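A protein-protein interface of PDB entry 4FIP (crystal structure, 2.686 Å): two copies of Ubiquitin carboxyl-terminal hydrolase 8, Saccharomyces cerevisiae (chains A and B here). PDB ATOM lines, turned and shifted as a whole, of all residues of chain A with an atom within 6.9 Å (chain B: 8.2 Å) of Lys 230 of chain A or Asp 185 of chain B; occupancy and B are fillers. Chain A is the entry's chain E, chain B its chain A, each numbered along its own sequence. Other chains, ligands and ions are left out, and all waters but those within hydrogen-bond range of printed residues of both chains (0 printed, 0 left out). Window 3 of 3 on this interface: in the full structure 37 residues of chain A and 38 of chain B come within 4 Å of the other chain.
OD1 of Asp 185 of chain B sits at hydrogen-bond distance from OG of Ser 183 of chain B (3.3 Å). The side-chain sulfur (SG) of Cys 227 of chain B is in hydrogen-bond range of the backbone carbonyl oxygen (O) of Asp 185 of chain B (3.2 Å). OG1 of Thr 226 of chain B sits at hydrogen-bond distance from O of Ile 222 of chain B (2.8 Å). O of Asp 185 of chain A is in hydrogen-bond range of SG of Cys 227 of chain A (3.1 Å).
Of chain B, only Asp 185 (3.3 Å), Thr 226 (3.2 Å) and Lys 230 (3.2 Å) come within 4 Å of Lys 230 of chain A. Asp 185 of chain B touches one residue of chain A. Printed residues of chain B within 4 Å of Thr 226 of chain A: Thr 226. Of the printed residues of chain B, Asp 185 of chain A touches Lys 230. The nearest residue of chain A that does not touch Asp 185 of chain B is Lys 186 of chain A (6.4 Å). The nearest printed residue of chain B that does not touch Trp 229 of chain A is Thr 226 of chain B (4.9 Å).
Asp 185 of chain A touches Lys 230 of chain B, and with the chains exchanged Lys 230 of chain A touches Asp 185 of chain B. Thr 226 of chain A touches its own counterpart, Thr 226 of chain B. Lys 230 of chain A touches Thr 226 of chain B, but with the chains exchanged Thr 226 of chain A does not touch Lys 230 of chain B (4.6 Å). Lys 230 of chain A touches its own counterpart, Lys 230 of chain B. 8 positions are printed for both chains. Of the 8 pairs that touch across the chains among the printed residues, 4 have their exchanged pair printed and touching as well.
Of the 22 printed residues of chain B, 5 touch a printed residue of chain A. Of the 11 printed residues of chain A, 5 touch a printed residue of chain B. Hydrophobic or aromatic side chains of chain A within 4 Å of the printed part of chain B: Trp 229.
CE of Lys 230 of chain B touches CB of Asp 185 of chain A, at 3.4 Å. CB of Thr 226 of chain A touches CG2 of Thr 226 of chain B, at 3.7 Å. CB of Trp 229 of chain A touches CG2 of Ile 222 of chain B, 3.7 Å away. Asp 185 of chain B touches Lys 230 of chain A. Thr 226 of chain B touches Lys 230 of chain A. Gln 233 of chain A touches Ile 222 of chain B.
OG1 of Thr 219 of chain B is in hydrogen-bond range of NE2 of Gln 233 of chain A (2.9 Å). The side-chain amino group (NZ) of Lys 230 of chain B sits close to the side-chain amino group (NZ) of Lys 230 of chain A (3.2 Å).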
ATOM      1  N   ASP A 185      10.291 -12.610  16.831  1.00  0.00           N
ATOM      2  CA  ASP A 185       9.486 -13.334  17.847  1.00  0.00           C
ATOM      3  C   ASP A 185       8.015 -12.951  17.799  1.00  0.00           C
ATOM      4  O   ASP A 185       7.171 -13.788  18.091  1.00  0.00           O
ATOM      5  CB  ASP A 185      10.015 -13.209  19.288  1.00  0.00           C
ATOM      6  CG  ASP A 185      10.698 -11.898  19.562  1.00  0.00           C
ATOM      7  OD1 ASP A 185      11.374 -11.380  18.652  1.00  0.00           O
ATOM      8  OD2 ASP A 185      10.583 -11.397  20.699  1.00  0.00           O
ATOM      9  N   LYS A 186       7.710 -11.706  17.430  1.00  0.00           N
ATOM     10  CA  LYS A 186       6.313 -11.260  17.285  1.00  0.00           C
ATOM     11  C   LYS A 186       5.764 -11.562  15.884  1.00  0.00           C
ATOM     12  O   LYS A 186       4.812 -12.328  15.765  1.00  0.00           O
ATOM     13  CB  LYS A 186       6.157  -9.773  17.655  1.00  0.00           C
ATOM     14  CG  LYS A 186       6.456  -9.455  19.134  1.00  0.00           C
ATOM     15  CD  LYS A 186       6.246  -7.973  19.471  1.00  0.00           C
ATOM     16  CE  LYS A 186       6.770  -7.588  20.855  1.00  0.00           C
ATOM     17  NZ  LYS A 186       6.632  -6.129  21.161  1.00  0.00           N
ATOM     18  N   LEU A 225       8.520 -21.255  14.766  1.00  0.00           N
ATOM     19  CA  LEU A 225       7.658 -22.145  15.542  1.00  0.00           C
ATOM     20  C   LEU A 225       6.908 -21.369  16.624  1.00  0.00           C
ATOM     21  O   LEU A 225       5.679 -21.439  16.704  1.00  0.00           O
ATOM     22  CB  LEU A 225       8.433 -23.291  16.186  1.00  0.00           C
ATOM     23  CG  LEU A 225       9.053 -24.287  15.211  1.00  0.00           C
ATOM     24  CD1 LEU A 225       9.955 -25.303  15.907  1.00  0.00           C
ATOM     25  CD2 LEU A 225       7.920 -24.946  14.465  1.00  0.00           C
ATOM     26  N   THR A 226       7.644 -20.612  17.438  1.00  0.00           N
ATOM     27  CA  THR A 226       7.007 -19.931  18.562  1.00  0.00           C
ATOM     28  C   THR A 226       5.915 -19.021  18.039  1.00  0.00           C
ATOM     29  O   THR A 226       4.813 -19.006  18.602  1.00  0.00           O
ATOM     30  CB  THR A 226       7.962 -19.136  19.506  1.00  0.00           C
ATOM     31  OG1 THR A 226       8.382 -17.899  18.904  1.00  0.00           O
ATOM     32  CG2 THR A 226       9.130 -19.973  19.920  1.00  0.00           C
ATOM     33  N   CYS A 227       6.192 -18.293  16.956  1.00  0.00           N
ATOM     34  CA  CYS A 227       5.145 -17.457  16.368  1.00  0.00           C
ATOM     35  C   CYS A 227       3.960 -18.332  16.044  1.00  0.00           C
ATOM     36  O   CYS A 227       2.871 -18.045  16.511  1.00  0.00           O
ATOM     37  CB  CYS A 227       5.630 -16.700  15.144  1.00  0.00           C
ATOM     38  SG  CYS A 227       6.930 -15.492  15.518  1.00  0.00           S
ATOM     39  N   ALA A 228       4.217 -19.441  15.338  1.00  0.00           N
ATOM     40  CA  ALA A 228       3.184 -20.413  14.903  1.00  0.00           C
ATOM     41  C   ALA A 228       2.286 -20.950  16.020  1.00  0.00           C
ATOM     42  O   ALA A 228       1.063 -20.818  15.943  1.00  0.00           O
ATOM     43  CB  ALA A 228       3.819 -21.587  14.169  1.00  0.00           C
ATOM     44  N   TRP A 229       2.901 -21.563  17.035  1.00  0.00           N
ATOM     45  CA  TRP A 229       2.167 -22.231  18.126  1.00  0.00           C
ATOM     46  C   TRP A 229       1.340 -21.286  18.936  1.00  0.00           C
ATOM     47  O   TRP A 229       0.295 -21.661  19.424  1.00  0.00           O
ATOM     48  CB  TRP A 229       3.116 -22.929  19.087  1.00  0.00           C
ATOM     49  CG  TRP A 229       3.912 -24.072  18.520  1.00  0.00           C
ATOM     50  CD1 TRP A 229       3.510 -25.018  17.579  1.00  0.00           C
ATOM     51  CD2 TRP A 229       5.283 -24.454  18.882  1.00  0.00           C
ATOM     52  NE1 TRP A 229       4.519 -25.918  17.325  1.00  0.00           N
ATOM     53  CE2 TRP A 229       5.603 -25.643  18.077  1.00  0.00           C
ATOM     54  CE3 TRP A 229       6.241 -23.947  19.757  1.00  0.00           C
ATOM     55  CZ2 TRP A 229       6.827 -26.267  18.153  1.00  0.00           C
ATOM     56  CZ3 TRP A 229       7.473 -24.586  19.838  1.00  0.00           C
ATOM     57  CH2 TRP A 229       7.763 -25.719  19.048  1.00  0.00           C
ATOM     58  N   LYS A 230       1.826 -20.067  19.126  1.00  0.00           N
ATOM     59  CA  LYS A 230       1.051 -19.026  19.776  1.00  0.00           C
ATOM     60  C   LYS A 230      -0.185 -18.671  18.945  1.00  0.00           C
ATOM     61  O   LYS A 230      -1.281 -18.588  19.488  1.00  0.00           O
ATOM     62  CB  LYS A 230       1.918 -17.788  20.035  1.00  0.00           C
ATOM     63  CG  LYS A 230       2.922 -18.011  21.165  1.00  0.00           C
ATOM     64  CD  LYS A 230       3.904 -16.851  21.363  1.00  0.00           C
ATOM     65  CE  LYS A 230       4.956 -17.186  22.428  1.00  0.00           C
ATOM     66  NZ  LYS A 230       5.856 -16.052  22.828  1.00  0.00           N
ATOM     67  N   ILE A 231      -0.018 -18.506  17.633  1.00  0.00           N
ATOM     68  CA  ILE A 231      -1.141 -18.146  16.737  1.00  0.00           C
ATOM     69  C   ILE A 231      -2.145 -19.284  16.581  1.00  0.00           C
ATOM     70  O   ILE A 231      -3.303 -19.030  16.299  1.00  0.00           O
ATOM     71  CB  ILE A 231      -0.710 -17.781  15.291  1.00  0.00           C
ATOM     72  CG1 ILE A 231       0.411 -16.750  15.235  1.00  0.00           C
ATOM     73  CG2 ILE A 231      -1.883 -17.191  14.547  1.00  0.00           C
ATOM     74  CD1 ILE A 231       1.130 -16.717  13.897  1.00  0.00           C
ATOM     75  N   ASN A 232      -1.687 -20.529  16.718  1.00  0.00           N
ATOM     76  CA  ASN A 232      -2.537 -21.705  16.520  1.00  0.00           C
ATOM     77  C   ASN A 232      -1.904 -22.978  17.081  1.00  0.00           C
ATOM     78  O   ASN A 232      -1.030 -23.587  16.451  1.00  0.00           O
ATOM     79  CB  ASN A 232      -2.857 -21.897  15.035  1.00  0.00           C
ATOM     80  CG  ASN A 232      -3.683 -23.150  14.767  1.00  0.00           C
ATOM     81  OD1 ASN A 232      -4.452 -23.604  15.626  1.00  0.00           O
ATOM     82  ND2 ASN A 232      -3.529 -23.717  13.569  1.00  0.00           N
ATOM     83  N   GLN A 233      -2.378 -23.393  18.250  1.00  0.00           N
ATOM     84  CA  GLN A 233      -1.718 -24.429  19.025  1.00  0.00           C
ATOM     85  C   GLN A 233      -1.969 -25.828  18.502  1.00  0.00           C
ATOM     86  O   GLN A 233      -1.257 -26.770  18.885  1.00  0.00           O
ATOM     87  CB  GLN A 233      -2.191 -24.375  20.449  1.00  0.00           C
ATOM     88  CG  GLN A 233      -2.048 -23.010  21.072  1.00  0.00           C
ATOM     89  CD  GLN A 233      -2.435 -23.054  22.513  1.00  0.00           C
ATOM     90  OE1 GLN A 233      -2.952 -24.072  22.984  1.00  0.00           O
ATOM     91  NE2 GLN A 233      -2.180 -21.964  23.234  1.00  0.00           N
ATOM     92  N   VAL B 181       6.090  -7.373  34.639  1.00  0.00           N
ATOM     93  CA  VAL B 181       5.745  -7.695  33.241  1.00  0.00           C
ATOM     94  C   VAL B 181       4.259  -8.029  33.071  1.00  0.00           C
ATOM     95  O   VAL B 181       3.621  -7.569  32.121  1.00  0.00           O
ATOM     96  CB  VAL B 181       6.518  -8.920  32.706  1.00  0.00           C
ATOM     97  CG1 VAL B 181       5.896  -9.388  31.397  1.00  0.00           C
ATOM     98  CG2 VAL B 181       7.998  -8.624  32.534  1.00  0.00           C
ATOM     99  N   ARG B 182       3.716  -8.860  33.961  1.00  0.00           N
ATOM    100  CA  ARG B 182       2.294  -9.255  33.902  1.00  0.00           C
ATOM    101  C   ARG B 182       1.878  -9.880  32.557  1.00  0.00           C
ATOM    102  O   ARG B 182       0.765  -9.647  32.099  1.00  0.00           O
ATOM    103  CB  ARG B 182       1.368  -8.056  34.188  1.00  0.00           C
ATOM    104  CG  ARG B 182       1.636  -7.297  35.480  1.00  0.00           C
ATOM    105  CD  ARG B 182       0.944  -7.927  36.684  1.00  0.00           C
ATOM    106  NE  ARG B 182       0.880  -7.004  37.824  1.00  0.00           N
ATOM    107  CZ  ARG B 182       0.285  -7.266  38.993  1.00  0.00           C
ATOM    108  NH1 ARG B 182      -0.311  -8.436  39.205  1.00  0.00           N
ATOM    109  NH2 ARG B 182       0.283  -6.352  39.962  1.00  0.00           N
ATOM    110  N   SER B 183       2.757 -10.649  31.914  1.00  0.00           N
ATOM    111  CA  SER B 183       2.326 -11.453  30.759  1.00  0.00           C
ATOM    112  C   SER B 183       3.207 -12.689  30.497  1.00  0.00           C
ATOM    113  O   SER B 183       4.439 -12.627  30.624  1.00  0.00           O
ATOM    114  CB  SER B 183       2.172 -10.614  29.474  1.00  0.00           C
ATOM    115  OG  SER B 183       3.272 -10.786  28.592  1.00  0.00           O
ATOM    116  N   PRO B 184       2.564 -13.811  30.112  1.00  0.00           N
ATOM    117  CA  PRO B 184       3.171 -15.132  29.966  1.00  0.00           C
ATOM    118  C   PRO B 184       4.253 -15.290  28.884  1.00  0.00           C
ATOM    119  O   PRO B 184       5.216 -16.029  29.088  1.00  0.00           O
ATOM    120  CB  PRO B 184       1.979 -16.018  29.609  1.00  0.00           C
ATOM    121  CG  PRO B 184       0.792 -15.285  30.079  1.00  0.00           C
ATOM    122  CD  PRO B 184       1.122 -13.861  29.826  1.00  0.00           C
ATOM    123  N   ASP B 185       4.098 -14.638  27.738  1.00  0.00           N
ATOM    124  CA  ASP B 185       5.098 -14.784  26.661  1.00  0.00           C
ATOM    125  C   ASP B 185       6.412 -14.083  26.982  1.00  0.00           C
ATOM    126  O   ASP B 185       7.453 -14.438  26.412  1.00  0.00           O
ATOM    127  CB  ASP B 185       4.561 -14.284  25.314  1.00  0.00           C
ATOM    128  CG  ASP B 185       3.871 -12.941  25.421  1.00  0.00           C
ATOM    129  OD1 ASP B 185       2.800 -12.879  26.065  1.00  0.00           O
ATOM    130  OD2 ASP B 185       4.395 -11.957  24.857  1.00  0.00           O
ATOM    131  N   LYS B 186       6.360 -13.113  27.900  1.00  0.00           N
ATOM    132  CA  LYS B 186       7.535 -12.335  28.295  1.00  0.00           C
ATOM    133  C   LYS B 186       8.158 -12.759  29.632  1.00  0.00           C
ATOM    134  O   LYS B 186       9.388 -12.781  29.747  1.00  0.00           O
ATOM    135  CB  LYS B 186       7.170 -10.858  28.354  1.00  0.00           C
ATOM    136  CG  LYS B 186       6.602 -10.293  27.055  1.00  0.00           C
ATOM    137  CD  LYS B 186       5.865  -8.977  27.282  1.00  0.00           C
ATOM    138  CE  LYS B 186       6.829  -7.833  27.555  1.00  0.00           C
ATOM    139  NZ  LYS B 186       6.081  -6.561  27.722  1.00  0.00           N
ATOM    140  N   CYS B 187       7.329 -13.088  30.638  1.00  0.00           N
ATOM    141  CA  CYS B 187       7.832 -13.503  31.985  1.00  0.00           C
ATOM    142  C   CYS B 187       7.638 -14.994  32.259  1.00  0.00           C
ATOM    143  O   CYS B 187       6.551 -15.533  32.082  1.00  0.00           O
ATOM    144  CB  CYS B 187       7.182 -12.691  33.123  1.00  0.00           C
ATOM    145  SG  CYS B 187       7.152 -13.561  34.718  1.00  0.00           S
ATOM    146  N   PHE B 188       8.696 -15.636  32.733  1.00  0.00           N
ATOM    147  CA  PHE B 188       8.740 -17.080  32.856  1.00  0.00           C
ATOM    148  C   PHE B 188       7.814 -17.538  33.978  1.00  0.00           C
ATOM    149  O   PHE B 188       7.100 -18.539  33.837  1.00  0.00           O
ATOM    150  CB  PHE B 188      10.179 -17.503  33.113  1.00  0.00           C
ATOM    151  CG  PHE B 188      10.389 -18.984  33.202  1.00  0.00           C
ATOM    152  CD1 PHE B 188      10.575 -19.736  32.078  1.00  0.00           C
ATOM    153  CD2 PHE B 188      10.475 -19.608  34.414  1.00  0.00           C
ATOM    154  CE1 PHE B 188      10.805 -21.097  32.146  1.00  0.00           C
ATOM    155  CE2 PHE B 188      10.707 -20.979  34.498  1.00  0.00           C
ATOM    156  CZ  PHE B 188      10.871 -21.729  33.357  1.00  0.00           C
ATOM    157  N   CYS B 190       5.253 -15.867  35.213  1.00  0.00           N
ATOM    158  CA  CYS B 190       3.923 -15.732  34.725  1.00  0.00           C
ATOM    159  C   CYS B 190       3.520 -17.008  33.949  1.00  0.00           C
ATOM    160  O   CYS B 190       2.447 -17.549  34.143  1.00  0.00           O
ATOM    161  CB  CYS B 190       3.807 -14.465  33.879  1.00  0.00           C
ATOM    162  SG  CYS B 190       3.719 -12.955  34.875  1.00  0.00           S
ATOM    163  N   ALA B 191       4.383 -17.506  33.086  1.00  0.00           N
ATOM    164  CA  ALA B 191       4.049 -18.719  32.353  1.00  0.00           C
ATOM    165  C   ALA B 191       3.857 -19.905  33.289  1.00  0.00           C
ATOM    166  O   ALA B 191       2.942 -20.701  33.075  1.00  0.00           O
ATOM    167  CB  ALA B 191       5.107 -19.042  31.308  1.00  0.00           C
ATOM    168  N   LYS B 194       0.505 -19.676  34.770  1.00  0.00           N
ATOM    169  CA  LYS B 194      -0.535 -19.999  33.814  1.00  0.00           C
ATOM    170  C   LYS B 194      -0.770 -21.512  33.706  1.00  0.00           C
ATOM    171  O   LYS B 194      -1.937 -21.970  33.589  1.00  0.00           O
ATOM    172  CB  LYS B 194      -0.200 -19.396  32.440  1.00  0.00           C
ATOM    173  CG  LYS B 194      -1.314 -19.592  31.410  1.00  0.00           C
ATOM    174  CD  LYS B 194      -1.410 -18.454  30.392  1.00  0.00           C
ATOM    175  CE  LYS B 194      -2.769 -18.437  29.703  1.00  0.00           C
ATOM    176  NZ  LYS B 194      -3.801 -17.784  30.554  1.00  0.00           N
ATOM    177  N   THR B 219      -1.647 -23.940  26.536  1.00  0.00           N
ATOM    178  CA  THR B 219      -1.124 -22.577  26.412  1.00  0.00           C
ATOM    179  C   THR B 219       0.012 -22.257  27.397  1.00  0.00           C
ATOM    180  O   THR B 219       1.014 -21.615  27.039  1.00  0.00           O
ATOM    181  CB  THR B 219      -2.259 -21.570  26.634  1.00  0.00           C
ATOM    182  OG1 THR B 219      -3.373 -21.978  25.838  1.00  0.00           O
ATOM    183  CG2 THR B 219      -1.837 -20.144  26.259  1.00  0.00           C
ATOM    184  N   GLY B 220      -0.157 -22.710  28.636  1.00  0.00           N
ATOM    185  CA  GLY B 220       0.806 -22.422  29.670  1.00  0.00           C
ATOM    186  C   GLY B 220       2.105 -23.012  29.219  1.00  0.00           C
ATOM    187  O   GLY B 220       3.135 -22.328  29.163  1.00  0.00           O
ATOM    188  N   ILE B 222       3.120 -23.915  26.326  1.00  0.00           N
ATOM    189  CA  ILE B 222       3.696 -23.451  25.082  1.00  0.00           C
ATOM    190  C   ILE B 222       4.362 -22.117  25.338  1.00  0.00           C
ATOM    191  O   ILE B 222       5.508 -21.917  24.975  1.00  0.00           O
ATOM    192  CB  ILE B 222       2.647 -23.373  23.960  1.00  0.00           C
ATOM    193  CG1 ILE B 222       2.262 -24.806  23.543  1.00  0.00           C
ATOM    194  CG2 ILE B 222       3.181 -22.557  22.772  1.00  0.00           C
ATOM    195  CD1 ILE B 222       1.088 -24.895  22.608  1.00  0.00           C
ATOM    196  N   TYR B 223       3.652 -21.214  25.996  1.00  0.00           N
ATOM    197  CA  TYR B 223       4.258 -19.978  26.471  1.00  0.00           C
ATOM    198  C   TYR B 223       5.539 -20.250  27.269  1.00  0.00           C
ATOM    199  O   TYR B 223       6.491 -19.484  27.173  1.00  0.00           O
ATOM    200  CB  TYR B 223       3.283 -19.221  27.368  1.00  0.00           C
ATOM    201  CG  TYR B 223       2.259 -18.319  26.703  1.00  0.00           C
ATOM    202  CD1 TYR B 223       2.615 -17.419  25.711  1.00  0.00           C
ATOM    203  CD2 TYR B 223       0.952 -18.297  27.150  1.00  0.00           C
ATOM    204  CE1 TYR B 223       1.681 -16.563  25.149  1.00  0.00           C
ATOM    205  CE2 TYR B 223       0.010 -17.447  26.603  1.00  0.00           C
ATOM    206  CZ  TYR B 223       0.379 -16.579  25.604  1.00  0.00           C
ATOM    207  OH  TYR B 223      -0.562 -15.731  25.068  1.00  0.00           O
ATOM    208  N   LEU B 224       5.564 -21.341  28.051  1.00  0.00           N
ATOM    209  CA  LEU B 224       6.753 -21.663  28.887  1.00  0.00           C
ATOM    210  C   LEU B 224       7.944 -22.196  28.099  1.00  0.00           C
ATOM    211  O   LEU B 224       9.067 -21.827  28.378  1.00  0.00           O
ATOM    212  CB  LEU B 224       6.412 -22.645  30.003  1.00  0.00           C
ATOM    213  CG  LEU B 224       7.426 -22.695  31.164  1.00  0.00           C
ATOM    214  CD1 LEU B 224       6.712 -22.928  32.489  1.00  0.00           C
ATOM    215  CD2 LEU B 224       8.509 -23.748  30.953  1.00  0.00           C
ATOM    216  N   LEU B 225       7.695 -23.095  27.155  1.00  0.00           N
ATOM    217  CA  LEU B 225       8.728 -23.574  26.247  1.00  0.00           C
ATOM    218  C   LEU B 225       9.413 -22.426  25.579  1.00  0.00           C
ATOM    219  O   LEU B 225      10.625 -22.340  25.585  1.00  0.00           O
ATOM    220  CB  LEU B 225       8.103 -24.415  25.154  1.00  0.00           C
ATOM    221  CG  LEU B 225       8.218 -25.889  25.492  1.00  0.00           C
ATOM    222  CD1 LEU B 225       6.959 -26.670  25.115  1.00  0.00           C
ATOM    223  CD2 LEU B 225       9.469 -26.393  24.786  1.00  0.00           C
ATOM    224  N   THR B 226       8.589 -21.559  24.998  1.00  0.00           N
ATOM    225  CA  THR B 226       9.009 -20.329  24.344  1.00  0.00           C
ATOM    226  C   THR B 226       9.833 -19.374  25.228  1.00  0.00           C
ATOM    227  O   THR B 226      10.914 -18.959  24.832  1.00  0.00           O
ATOM    228  CB  THR B 226       7.766 -19.563  23.850  1.00  0.00           C
ATOM    229  OG1 THR B 226       6.971 -20.436  23.034  1.00  0.00           O
ATOM    230  CG2 THR B 226       8.165 -18.309  23.076  1.00  0.00           C
ATOM    231  N   CYS B 227       9.294 -18.992  26.385  1.00  0.00           N
ATOM    232  CA  CYS B 227      10.042 -18.186  27.355  1.00  0.00           C
ATOM    233  C   CYS B 227      11.365 -18.820  27.704  1.00  0.00           C
ATOM    234  O   CYS B 227      12.319 -18.108  27.952  1.00  0.00           O
ATOM    235  CB  CYS B 227       9.273 -17.985  28.661  1.00  0.00           C
ATOM    236  SG  CYS B 227       8.140 -16.584  28.648  1.00  0.00           S
ATOM    237  N   ALA B 228      11.428 -20.148  27.731  1.00  0.00           N
ATOM    238  CA  ALA B 228      12.656 -20.838  28.130  1.00  0.00           C
ATOM    239  C   ALA B 228      13.759 -20.635  27.088  1.00  0.00           C
ATOM    240  O   ALA B 228      14.908 -20.302  27.404  1.00  0.00           O
ATOM    241  CB  ALA B 228      12.401 -22.325  28.371  1.00  0.00           C
ATOM    242  N   LYS B 230      13.856 -18.367  24.508  1.00  0.00           N
ATOM    243  CA  LYS B 230      14.220 -16.952  24.407  1.00  0.00           C
ATOM    244  C   LYS B 230      15.300 -16.613  25.421  1.00  0.00           C
ATOM    245  O   LYS B 230      16.312 -16.030  25.054  1.00  0.00           O
ATOM    246  CB  LYS B 230      13.005 -16.030  24.578  1.00  0.00           C
ATOM    247  CG  LYS B 230      12.244 -15.837  23.276  1.00  0.00           C
ATOM    248  CD  LYS B 230      10.883 -15.200  23.480  1.00  0.00           C
ATOM    249  CE  LYS B 230      10.135 -15.089  22.156  1.00  0.00           C
ATOM    250  NZ  LYS B 230       8.695 -14.762  22.378  1.00  0.00           N
ATOM    251  N   ILE B 231      15.084 -17.018  26.677  1.00  0.00           N
ATOM    252  CA  ILE B 231      16.036 -16.790  27.771  1.00  0.00           C
ATOM    253  C   ILE B 231      17.357 -17.516  27.500  1.00  0.00           C
ATOM    254  O   ILE B 231      18.432 -16.950  27.731  1.00  0.00           O
ATOM    255  CB  ILE B 231      15.454 -17.247  29.140  1.00  0.00           C
ATOM    256  CG1 ILE B 231      14.264 -16.377  29.562  1.00  0.00           C
ATOM    257  CG2 ILE B 231      16.507 -17.178  30.248  1.00  0.00           C
ATOM    258  CD1 ILE B 231      13.485 -16.913  30.751  1.00  0.00           C
